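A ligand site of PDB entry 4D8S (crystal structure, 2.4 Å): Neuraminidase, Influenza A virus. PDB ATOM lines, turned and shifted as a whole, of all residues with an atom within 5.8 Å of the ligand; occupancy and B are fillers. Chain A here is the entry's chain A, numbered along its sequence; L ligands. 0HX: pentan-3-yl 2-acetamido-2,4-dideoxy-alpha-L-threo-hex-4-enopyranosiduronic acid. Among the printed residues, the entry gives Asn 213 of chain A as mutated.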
ATOM      1  N   ARG A  36      14.741 -12.395 -14.715  1.00  0.00           N
ATOM      2  CA  ARG A  36      15.560 -11.265 -14.317  1.00  0.00           C
ATOM      3  C   ARG A  36      16.996 -11.700 -14.501  1.00  0.00           C
ATOM      4  O   ARG A  36      17.281 -12.893 -14.613  1.00  0.00           O
ATOM      5  CB  ARG A  36      15.293 -10.895 -12.852  1.00  0.00           C
ATOM      6  CG  ARG A  36      15.793  -9.516 -12.469  1.00  0.00           C
ATOM      7  CD  ARG A  36      14.984  -8.419 -13.147  1.00  0.00           C
ATOM      8  NE  ARG A  36      15.007  -7.172 -12.402  1.00  0.00           N
ATOM      9  CZ  ARG A  36      16.089  -6.687 -11.790  1.00  0.00           C
ATOM     10  NH1 ARG A  36      15.957  -5.937 -10.703  1.00  0.00           N
ATOM     11  NH2 ARG A  36      17.295  -6.940 -12.273  1.00  0.00           N
ATOM     12  N   GLU A  37      17.913 -10.737 -14.585  1.00  0.00           N
ATOM     13  CA  GLU A  37      19.339 -11.015 -14.775  1.00  0.00           C
ATOM     14  C   GLU A  37      19.664 -11.807 -16.048  1.00  0.00           C
ATOM     15  O   GLU A  37      20.435 -12.765 -16.015  1.00  0.00           O
ATOM     16  CB  GLU A  37      19.900 -11.743 -13.552  1.00  0.00           C
ATOM     17  CG  GLU A  37      19.996 -10.877 -12.302  1.00  0.00           C
ATOM     18  CD  GLU A  37      18.683 -10.822 -11.536  1.00  0.00           C
ATOM     19  OE1 GLU A  37      17.899 -11.789 -11.627  1.00  0.00           O
ATOM     20  OE2 GLU A  37      18.439  -9.811 -10.844  1.00  0.00           O
ATOM     21  N   VAL A  67       8.952  -9.349  -7.329  1.00  0.00           N
ATOM     22  CA  VAL A  67       9.916  -8.300  -7.068  1.00  0.00           C
ATOM     23  C   VAL A  67      11.003  -8.903  -6.192  1.00  0.00           C
ATOM     24  O   VAL A  67      12.198  -8.738  -6.471  1.00  0.00           O
ATOM     25  CB  VAL A  67       9.296  -7.056  -6.369  1.00  0.00           C
ATOM     26  CG1 VAL A  67       8.266  -6.423  -7.255  1.00  0.00           C
ATOM     27  CG2 VAL A  67       8.673  -7.443  -5.042  1.00  0.00           C
ATOM     28  N   ASP A  69      13.879 -10.531  -4.522  1.00  0.00           N
ATOM     29  CA  ASP A  69      15.098 -10.846  -5.243  1.00  0.00           C
ATOM     30  C   ASP A  69      15.640 -12.249  -4.948  1.00  0.00           C
ATOM     31  O   ASP A  69      16.376 -12.814  -5.752  1.00  0.00           O
ATOM     32  CB  ASP A  69      16.173  -9.783  -4.948  1.00  0.00           C
ATOM     33  CG  ASP A  69      15.697  -8.355  -5.257  1.00  0.00           C
ATOM     34  OD1 ASP A  69      14.842  -8.201  -6.162  1.00  0.00           O
ATOM     35  OD2 ASP A  69      16.171  -7.394  -4.598  1.00  0.00           O
ATOM     36  N   ARG A  70      15.264 -12.819  -3.794  1.00  0.00           N
ATOM     37  CA  ARG A  70      15.828 -14.102  -3.368  1.00  0.00           C
ATOM     38  C   ARG A  70      14.786 -15.105  -2.868  1.00  0.00           C
ATOM     39  O   ARG A  70      14.311 -14.994  -1.743  1.00  0.00           O
ATOM     40  CB  ARG A  70      16.874 -13.878  -2.255  1.00  0.00           C
ATOM     41  CG  ARG A  70      18.175 -13.218  -2.720  1.00  0.00           C
ATOM     42  CD  ARG A  70      19.075 -12.868  -1.534  1.00  0.00           C
ATOM     43  NE  ARG A  70      18.330 -12.077  -0.557  1.00  0.00           N
ATOM     44  CZ  ARG A  70      18.215 -10.748  -0.601  1.00  0.00           C
ATOM     45  NH1 ARG A  70      17.510 -10.111   0.330  1.00  0.00           N
ATOM     46  NH2 ARG A  70      18.804 -10.063  -1.566  1.00  0.00           N
ATOM     47  N   ARG A  74      13.797 -19.845  -7.185  1.00  0.00           N
ATOM     48  CA  ARG A  74      14.662 -19.188  -8.153  1.00  0.00           C
ATOM     49  C   ARG A  74      15.624 -20.183  -8.804  1.00  0.00           C
ATOM     50  O   ARG A  74      16.310 -20.932  -8.114  1.00  0.00           O
ATOM     51  CB  ARG A  74      15.476 -18.090  -7.467  1.00  0.00           C
ATOM     52  CG  ARG A  74      15.814 -16.909  -8.353  1.00  0.00           C
ATOM     53  CD  ARG A  74      14.734 -15.860  -8.265  1.00  0.00           C
ATOM     54  NE  ARG A  74      14.786 -14.970  -9.410  1.00  0.00           N
ATOM     55  CZ  ARG A  74      15.452 -13.818  -9.436  1.00  0.00           C
ATOM     56  NH1 ARG A  74      15.426 -13.076 -10.542  1.00  0.00           N
ATOM     57  NH2 ARG A  74      16.125 -13.414  -8.370  1.00  0.00           N
ATOM     58  N   TRP A  97      19.577 -17.640  -6.925  1.00  0.00           N
ATOM     59  CA  TRP A  97      19.066 -16.273  -6.860  1.00  0.00           C
ATOM     60  C   TRP A  97      20.160 -15.249  -7.145  1.00  0.00           C
ATOM     61  O   TRP A  97      19.969 -14.042  -6.982  1.00  0.00           O
ATOM     62  CB  TRP A  97      18.343 -15.975  -5.540  1.00  0.00           C
ATOM     63  CG  TRP A  97      18.945 -16.585  -4.289  1.00  0.00           C
ATOM     64  CD1 TRP A  97      18.499 -17.701  -3.630  1.00  0.00           C
ATOM     65  CD2 TRP A  97      20.048 -16.097  -3.526  1.00  0.00           C
ATOM     66  NE1 TRP A  97      19.271 -17.942  -2.515  1.00  0.00           N
ATOM     67  CE2 TRP A  97      20.237 -16.975  -2.436  1.00  0.00           C
ATOM     68  CE3 TRP A  97      20.923 -15.006  -3.669  1.00  0.00           C
ATOM     69  CZ2 TRP A  97      21.253 -16.786  -1.493  1.00  0.00           C
ATOM     70  CZ3 TRP A  97      21.916 -14.830  -2.739  1.00  0.00           C
ATOM     71  CH2 TRP A  97      22.077 -15.709  -1.660  1.00  0.00           C
ATOM     72  N   SER A  98      21.315 -15.755  -7.568  1.00  0.00           N
ATOM     73  CA  SER A  98      22.465 -14.963  -8.011  1.00  0.00           C
ATOM     74  C   SER A  98      23.380 -15.942  -8.751  1.00  0.00           C
ATOM     75  O   SER A  98      23.494 -17.112  -8.367  1.00  0.00           O
ATOM     76  CB  SER A  98      23.174 -14.345  -6.799  1.00  0.00           C
ATOM     77  OG  SER A  98      24.366 -13.682  -7.182  1.00  0.00           O
ATOM     78  N   ILE A 141      24.658 -12.911   2.535  1.00  0.00           N
ATOM     79  CA  ILE A 141      24.275 -12.973   1.122  1.00  0.00           C
ATOM     80  C   ILE A 141      25.387 -13.194   0.077  1.00  0.00           C
ATOM     81  O   ILE A 141      25.560 -12.383  -0.824  1.00  0.00           O
ATOM     82  CB  ILE A 141      23.470 -11.719   0.708  1.00  0.00           C
ATOM     83  CG1 ILE A 141      22.369 -11.430   1.727  1.00  0.00           C
ATOM     84  CG2 ILE A 141      22.882 -11.890  -0.686  1.00  0.00           C
ATOM     85  CD1 ILE A 141      21.403 -10.354   1.286  1.00  0.00           C
ATOM     86  N   LEU A 142      26.117 -14.294   0.210  1.00  0.00           N
ATOM     87  CA  LEU A 142      27.045 -14.680  -0.844  1.00  0.00           C
ATOM     88  C   LEU A 142      26.363 -14.422  -2.182  1.00  0.00           C
ATOM     89  O   LEU A 142      25.199 -14.810  -2.372  1.00  0.00           O
ATOM     90  CB  LEU A 142      27.453 -16.154  -0.734  1.00  0.00           C
ATOM     91  CG  LEU A 142      28.512 -16.660  -1.717  1.00  0.00           C
ATOM     92  CD1 LEU A 142      29.866 -16.028  -1.415  1.00  0.00           C
ATOM     93  CD2 LEU A 142      28.594 -18.171  -1.661  1.00  0.00           C
ATOM     94  N   ARG A 143      27.068 -13.778  -3.093  1.00  0.00           N
ATOM     95  CA  ARG A 143      26.508 -13.456  -4.401  1.00  0.00           C
ATOM     96  C   ARG A 143      27.592 -13.364  -5.478  1.00  0.00           C
ATOM     97  O   ARG A 143      28.781 -13.505  -5.181  1.00  0.00           O
ATOM     98  CB  ARG A 143      25.811 -12.093  -4.365  1.00  0.00           C
ATOM     99  CG  ARG A 143      26.538 -11.037  -3.542  1.00  0.00           C
ATOM    100  CD  ARG A 143      25.681  -9.810  -3.321  1.00  0.00           C
ATOM    101  NE  ARG A 143      26.346  -8.807  -2.508  1.00  0.00           N
ATOM    102  CZ  ARG A 143      26.331  -8.780  -1.186  1.00  0.00           C
ATOM    103  NH1 ARG A 143      26.974  -7.834  -0.524  1.00  0.00           N
ATOM    104  NH2 ARG A 143      25.674  -9.718  -0.505  1.00  0.00           N
ATOM    105  N   GLU A 146      26.026 -11.859 -11.928  1.00  0.00           N
ATOM    106  CA  GLU A 146      24.829 -11.679 -12.722  1.00  0.00           C
ATOM    107  C   GLU A 146      25.240 -11.327 -14.143  1.00  0.00           C
ATOM    108  O   GLU A 146      24.520 -10.611 -14.852  1.00  0.00           O
ATOM    109  CB  GLU A 146      23.939 -10.584 -12.160  1.00  0.00           C
ATOM    110  CG  GLU A 146      23.869 -10.550 -10.648  1.00  0.00           C
ATOM    111  CD  GLU A 146      23.376 -11.837 -10.026  1.00  0.00           C
ATOM    112  OE1 GLU A 146      23.249 -12.852 -10.745  1.00  0.00           O
ATOM    113  OE2 GLU A 146      23.113 -11.843  -8.806  1.00  0.00           O
ATOM    114  N   ALA A 165      25.198  -4.580   1.755  1.00  0.00           N
ATOM    115  CA  ALA A 165      25.132  -3.996   0.419  1.00  0.00           C
ATOM    116  C   ALA A 165      25.091  -2.477   0.465  1.00  0.00           C
ATOM    117  O   ALA A 165      25.143  -1.834  -0.584  1.00  0.00           O
ATOM    118  CB  ALA A 165      23.937  -4.542  -0.333  1.00  0.00           C
ATOM    119  N   GLU A 195      30.274  -4.704  -6.472  1.00  0.00           N
ATOM    120  CA  GLU A 195      29.105  -5.551  -6.755  1.00  0.00           C
ATOM    121  C   GLU A 195      29.054  -5.955  -8.223  1.00  0.00           C
ATOM    122  O   GLU A 195      29.436  -5.183  -9.103  1.00  0.00           O
ATOM    123  CB  GLU A 195      27.816  -4.808  -6.433  1.00  0.00           C
ATOM    124  CG  GLU A 195      27.603  -4.546  -4.966  1.00  0.00           C
ATOM    125  CD  GLU A 195      27.342  -5.808  -4.182  1.00  0.00           C
ATOM    126  OE1 GLU A 195      27.650  -5.822  -2.975  1.00  0.00           O
ATOM    127  OE2 GLU A 195      26.835  -6.798  -4.765  1.00  0.00           O
ATOM    128  N   GLU A 196      28.597  -7.177  -8.463  1.00  0.00           N
ATOM    129  CA  GLU A 196      28.192  -7.591  -9.804  1.00  0.00           C
ATOM    130  C   GLU A 196      29.117  -7.054 -10.900  1.00  0.00           C
ATOM    131  O   GLU A 196      28.751  -6.137 -11.629  1.00  0.00           O
ATOM    132  CB  GLU A 196      26.764  -7.126 -10.059  1.00  0.00           C
ATOM    133  CG  GLU A 196      25.720  -7.760  -9.134  1.00  0.00           C
ATOM    134  CD  GLU A 196      24.397  -6.994  -9.129  1.00  0.00           C
ATOM    135  OE1 GLU A 196      24.388  -5.819  -9.551  1.00  0.00           O
ATOM    136  OE2 GLU A 196      23.362  -7.575  -8.706  1.00  0.00           O
ATOM    137  N   ARG A 211      29.986  -2.502  -9.662  1.00  0.00           N
ATOM    138  CA  ARG A 211      29.019  -1.595  -9.041  1.00  0.00           C
ATOM    139  C   ARG A 211      29.301  -1.212  -7.581  1.00  0.00           C
ATOM    140  O   ARG A 211      29.198  -2.038  -6.662  1.00  0.00           O
ATOM    141  CB  ARG A 211      27.659  -2.281  -9.128  1.00  0.00           C
ATOM    142  CG  ARG A 211      26.622  -1.729  -8.142  1.00  0.00           C
ATOM    143  CD  ARG A 211      25.342  -2.577  -8.152  1.00  0.00           C
ATOM    144  NE  ARG A 211      24.218  -1.926  -7.475  1.00  0.00           N
ATOM    145  CZ  ARG A 211      22.967  -2.365  -7.516  1.00  0.00           C
ATOM    146  NH1 ARG A 211      22.005  -1.709  -6.875  1.00  0.00           N
ATOM    147  NH2 ARG A 211      22.662  -3.456  -8.214  1.00  0.00           N
ATOM    148  N   ASN A 213      27.893   0.100  -4.562  1.00  0.00           N
ATOM    149  CA  ASN A 213      26.524   0.277  -4.083  1.00  0.00           C
ATOM    150  C   ASN A 213      26.516   1.034  -2.754  1.00  0.00           C
ATOM    151  O   ASN A 213      25.491   1.131  -2.080  1.00  0.00           O
ATOM    152  CB  ASN A 213      25.826  -1.075  -3.950  1.00  0.00           C
ATOM    153  CG  ASN A 213      24.306  -0.954  -3.981  1.00  0.00           C
ATOM    154  OD1 ASN A 213      23.769  -0.598  -5.138  1.00  0.00           O
ATOM    155  ND2 ASN A 213      23.638  -1.172  -2.967  1.00  0.00           N
ATOM    156  N   GLY A 265      22.817   1.967  -6.700  1.00  0.00           N
ATOM    157  CA  GLY A 265      23.525   1.699  -7.940  1.00  0.00           C
ATOM    158  C   GLY A 265      22.770   0.742  -8.838  1.00  0.00           C
ATOM    159  O   GLY A 265      21.587   0.463  -8.639  1.00  0.00           O
ATOM    160  N   VAL A 266      23.472   0.236  -9.853  1.00  0.00           N
ATOM    161  CA  VAL A 266      22.921  -0.723 -10.792  1.00  0.00           C
ATOM    162  C   VAL A 266      24.054  -1.323 -11.611  1.00  0.00           C
ATOM    163  O   VAL A 266      25.060  -0.662 -11.864  1.00  0.00           O
ATOM    164  CB  VAL A 266      21.903  -0.062 -11.746  1.00  0.00           C
ATOM    165  CG1 VAL A 266      22.585   1.032 -12.563  1.00  0.00           C
ATOM    166  CG2 VAL A 266      21.263  -1.099 -12.642  1.00  0.00           C
ATOM    167  N   ARG A 288      16.024   4.174 -13.768  1.00  0.00           N
ATOM    168  CA  ARG A 288      16.496   3.155 -14.690  1.00  0.00           C
ATOM    169  C   ARG A 288      15.748   3.280 -16.005  1.00  0.00           C
ATOM    170  O   ARG A 288      15.036   2.366 -16.419  1.00  0.00           O
ATOM    171  CB  ARG A 288      16.306   1.748 -14.101  1.00  0.00           C
ATOM    172  CG  ARG A 288      17.270   1.417 -12.980  1.00  0.00           C
ATOM    173  CD  ARG A 288      17.055   0.005 -12.425  1.00  0.00           C
ATOM    174  NE  ARG A 288      17.969  -0.274 -11.317  1.00  0.00           N
ATOM    175  CZ  ARG A 288      17.959  -1.384 -10.581  1.00  0.00           C
ATOM    176  NH1 ARG A 288      18.837  -1.537  -9.609  1.00  0.00           N
ATOM    177  NH2 ARG A 288      17.058  -2.345 -10.811  1.00  0.00           N
ATOM    178  N   TYR A 322      19.681  -3.491 -15.739  1.00  0.00           N
ATOM    179  CA  TYR A 322      21.013  -4.044 -15.833  1.00  0.00           C
ATOM    180  C   TYR A 322      21.571  -3.950 -17.253  1.00  0.00           C
ATOM    181  O   TYR A 322      20.835  -3.758 -18.233  1.00  0.00           O
ATOM    182  CB  TYR A 322      21.044  -5.506 -15.365  1.00  0.00           C
ATOM    183  CG  TYR A 322      21.144  -5.674 -13.861  1.00  0.00           C
ATOM    184  CD1 TYR A 322      20.925  -4.606 -13.008  1.00  0.00           C
ATOM    185  CD2 TYR A 322      21.480  -6.908 -13.290  1.00  0.00           C
ATOM    186  CE1 TYR A 322      21.016  -4.754 -11.618  1.00  0.00           C
ATOM    187  CE2 TYR A 322      21.585  -7.064 -11.915  1.00  0.00           C
ATOM    188  CZ  TYR A 322      21.348  -5.992 -11.088  1.00  0.00           C
ATOM    189  OH  TYR A 322      21.444  -6.136  -9.721  1.00  0.00           O
ATOM    190  N   ILE A 347      13.769  -3.797 -17.546  1.00  0.00           N
ATOM    191  CA  ILE A 347      12.797  -4.240 -16.541  1.00  0.00           C
ATOM    192  C   ILE A 347      11.426  -3.577 -16.699  1.00  0.00           C
ATOM    193  O   ILE A 347      11.320  -2.438 -17.118  1.00  0.00           O
ATOM    194  CB  ILE A 347      13.280  -3.967 -15.120  1.00  0.00           C
ATOM    195  CG1 ILE A 347      14.774  -4.274 -15.017  1.00  0.00           C
ATOM    196  CG2 ILE A 347      12.464  -4.771 -14.117  1.00  0.00           C
ATOM    197  CD1 ILE A 347      15.341  -4.073 -13.626  1.00  0.00           C
HETATM  198  C14 0HX L   1      21.830  -4.838  -3.934  1.00  0.00           C
HETATM  199  C15 0HX L   1      21.267  -3.471  -4.307  1.00  0.00           C
HETATM  200  C1  0HX L   1      20.491  -7.134  -6.216  1.00  0.00           C
HETATM  201  C2  0HX L   1      19.627  -8.384  -6.225  1.00  0.00           C
HETATM  202  C5  0HX L   1      18.974  -5.989  -7.575  1.00  0.00           C
HETATM  203  C6  0HX L   1      18.577  -4.636  -8.177  1.00  0.00           C
HETATM  204  C4  0HX L   1      18.537  -7.182  -8.151  1.00  0.00           C
HETATM  205  C3  0HX L   1      18.962  -8.541  -7.591  1.00  0.00           C
HETATM  206  C7  0HX L   1      20.405 -10.361  -4.941  1.00  0.00           C
HETATM  207  C8  0HX L   1      21.396 -11.527  -4.965  1.00  0.00           C
HETATM  208  N2  0HX L   1      20.471  -9.562  -5.995  1.00  0.00           N
HETATM  209  C13 0HX L   1      21.897  -5.764  -5.136  1.00  0.00           C
HETATM  210  C11 0HX L   1      24.270  -5.030  -5.357  1.00  0.00           C
HETATM  211  C12 0HX L   1      23.334  -6.248  -5.352  1.00  0.00           C
HETATM  212  O1  0HX L   1      21.047  -6.879  -4.927  1.00  0.00           O
HETATM  213  O5  0HX L   1      19.718  -5.976  -6.450  1.00  0.00           O
HETATM  214  O6B 0HX L   1      17.706  -4.582  -9.066  1.00  0.00           O
HETATM  215  O6A 0HX L   1      19.177  -3.630  -7.744  1.00  0.00           O
HETATM  216  O3  0HX L   1      17.832  -9.407  -7.516  1.00  0.00           O
HETATM  217  O6  0HX L   1      19.647 -10.203  -3.991  1.00  0.00           O
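Trp 97 touches the ligand (O to C8, 3.5 Å). CB of Ser 98 touches C8 of the ligand, 3.8 Å away. OE2 of Glu 195 touches C11 of the ligand, at 3.2 Å. Glu 196 touches the ligand (OE2 to C12, 3.6 Å). ND2 of Asn 213 touches C15 of the ligand, at 3.6 Å. Tyr 322 touches the ligand (OH to C5, 3.3 Å). Hydrophobic or aromatic side chains within 4 Å of the ligand: Trp 97. Of the 22 residues printed, 12 come within 4 Å of the ligand.
The side-chain carboxylate (OE2) of Glu 37 lies within salt-bridge range of the guanidinium group (NH2) of Arg 36, 3.4 Å away. The guanidinium group (NH2) of Arg 211 is in hydrogen-bond range of the side-chain hydroxyl (OH) of Tyr 322 (3.3 Å). The backbone carbonyl oxygen (O) of Val 67 sits close to the side-chain carboxylate (OD1) of Asp 69 (2.7 Å). The backbone NH of Gly 265 lies within hydrogen-bond range of the side-chain amide oxygen of Asn 213 (3.2 Å). The backbone carbonyl oxygen of Asp 69 lies within hydrogen-bond range of the guanidinium group of Arg 74, at 2.7 Å. OE1 of Glu 37 lies within salt-bridge range of NH1 of Arg 74 (3.0 Å). The side-chain hydroxyl of Ser 98 sits at hydrogen-bond distance from the side-chain carboxylate of Glu 146, 2.8 Å away. The backbone carbonyl oxygen (O) of Glu 195 is in hydrogen-bond range of the backbone NH (N) of Arg 211 (2.8 Å).
The guanidinium group (NH2) of Arg 70 sits at hydrogen-bond distance from an oxygen (O6) of the ligand, at 2.6 Å. O3 of the ligand sits close to OD1 of Asp 69 (3.5 Å). NH2 of Arg 211 is in salt-bridge range of O6A of the ligand, at 3.5 Å. An oxygen (O3) of the ligand sits at hydrogen-bond distance from the side-chain carboxylate (OE2) of Glu 37 (3.4 Å). The guanidinium group (NH1) of Arg 288 is in salt-bridge range of an oxygen (O6A) of the ligand (2.8 Å). The guanidinium group (NH1) of Arg 36 lies within salt-bridge range of an oxygen (O6B) of the ligand (2.8 Å).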
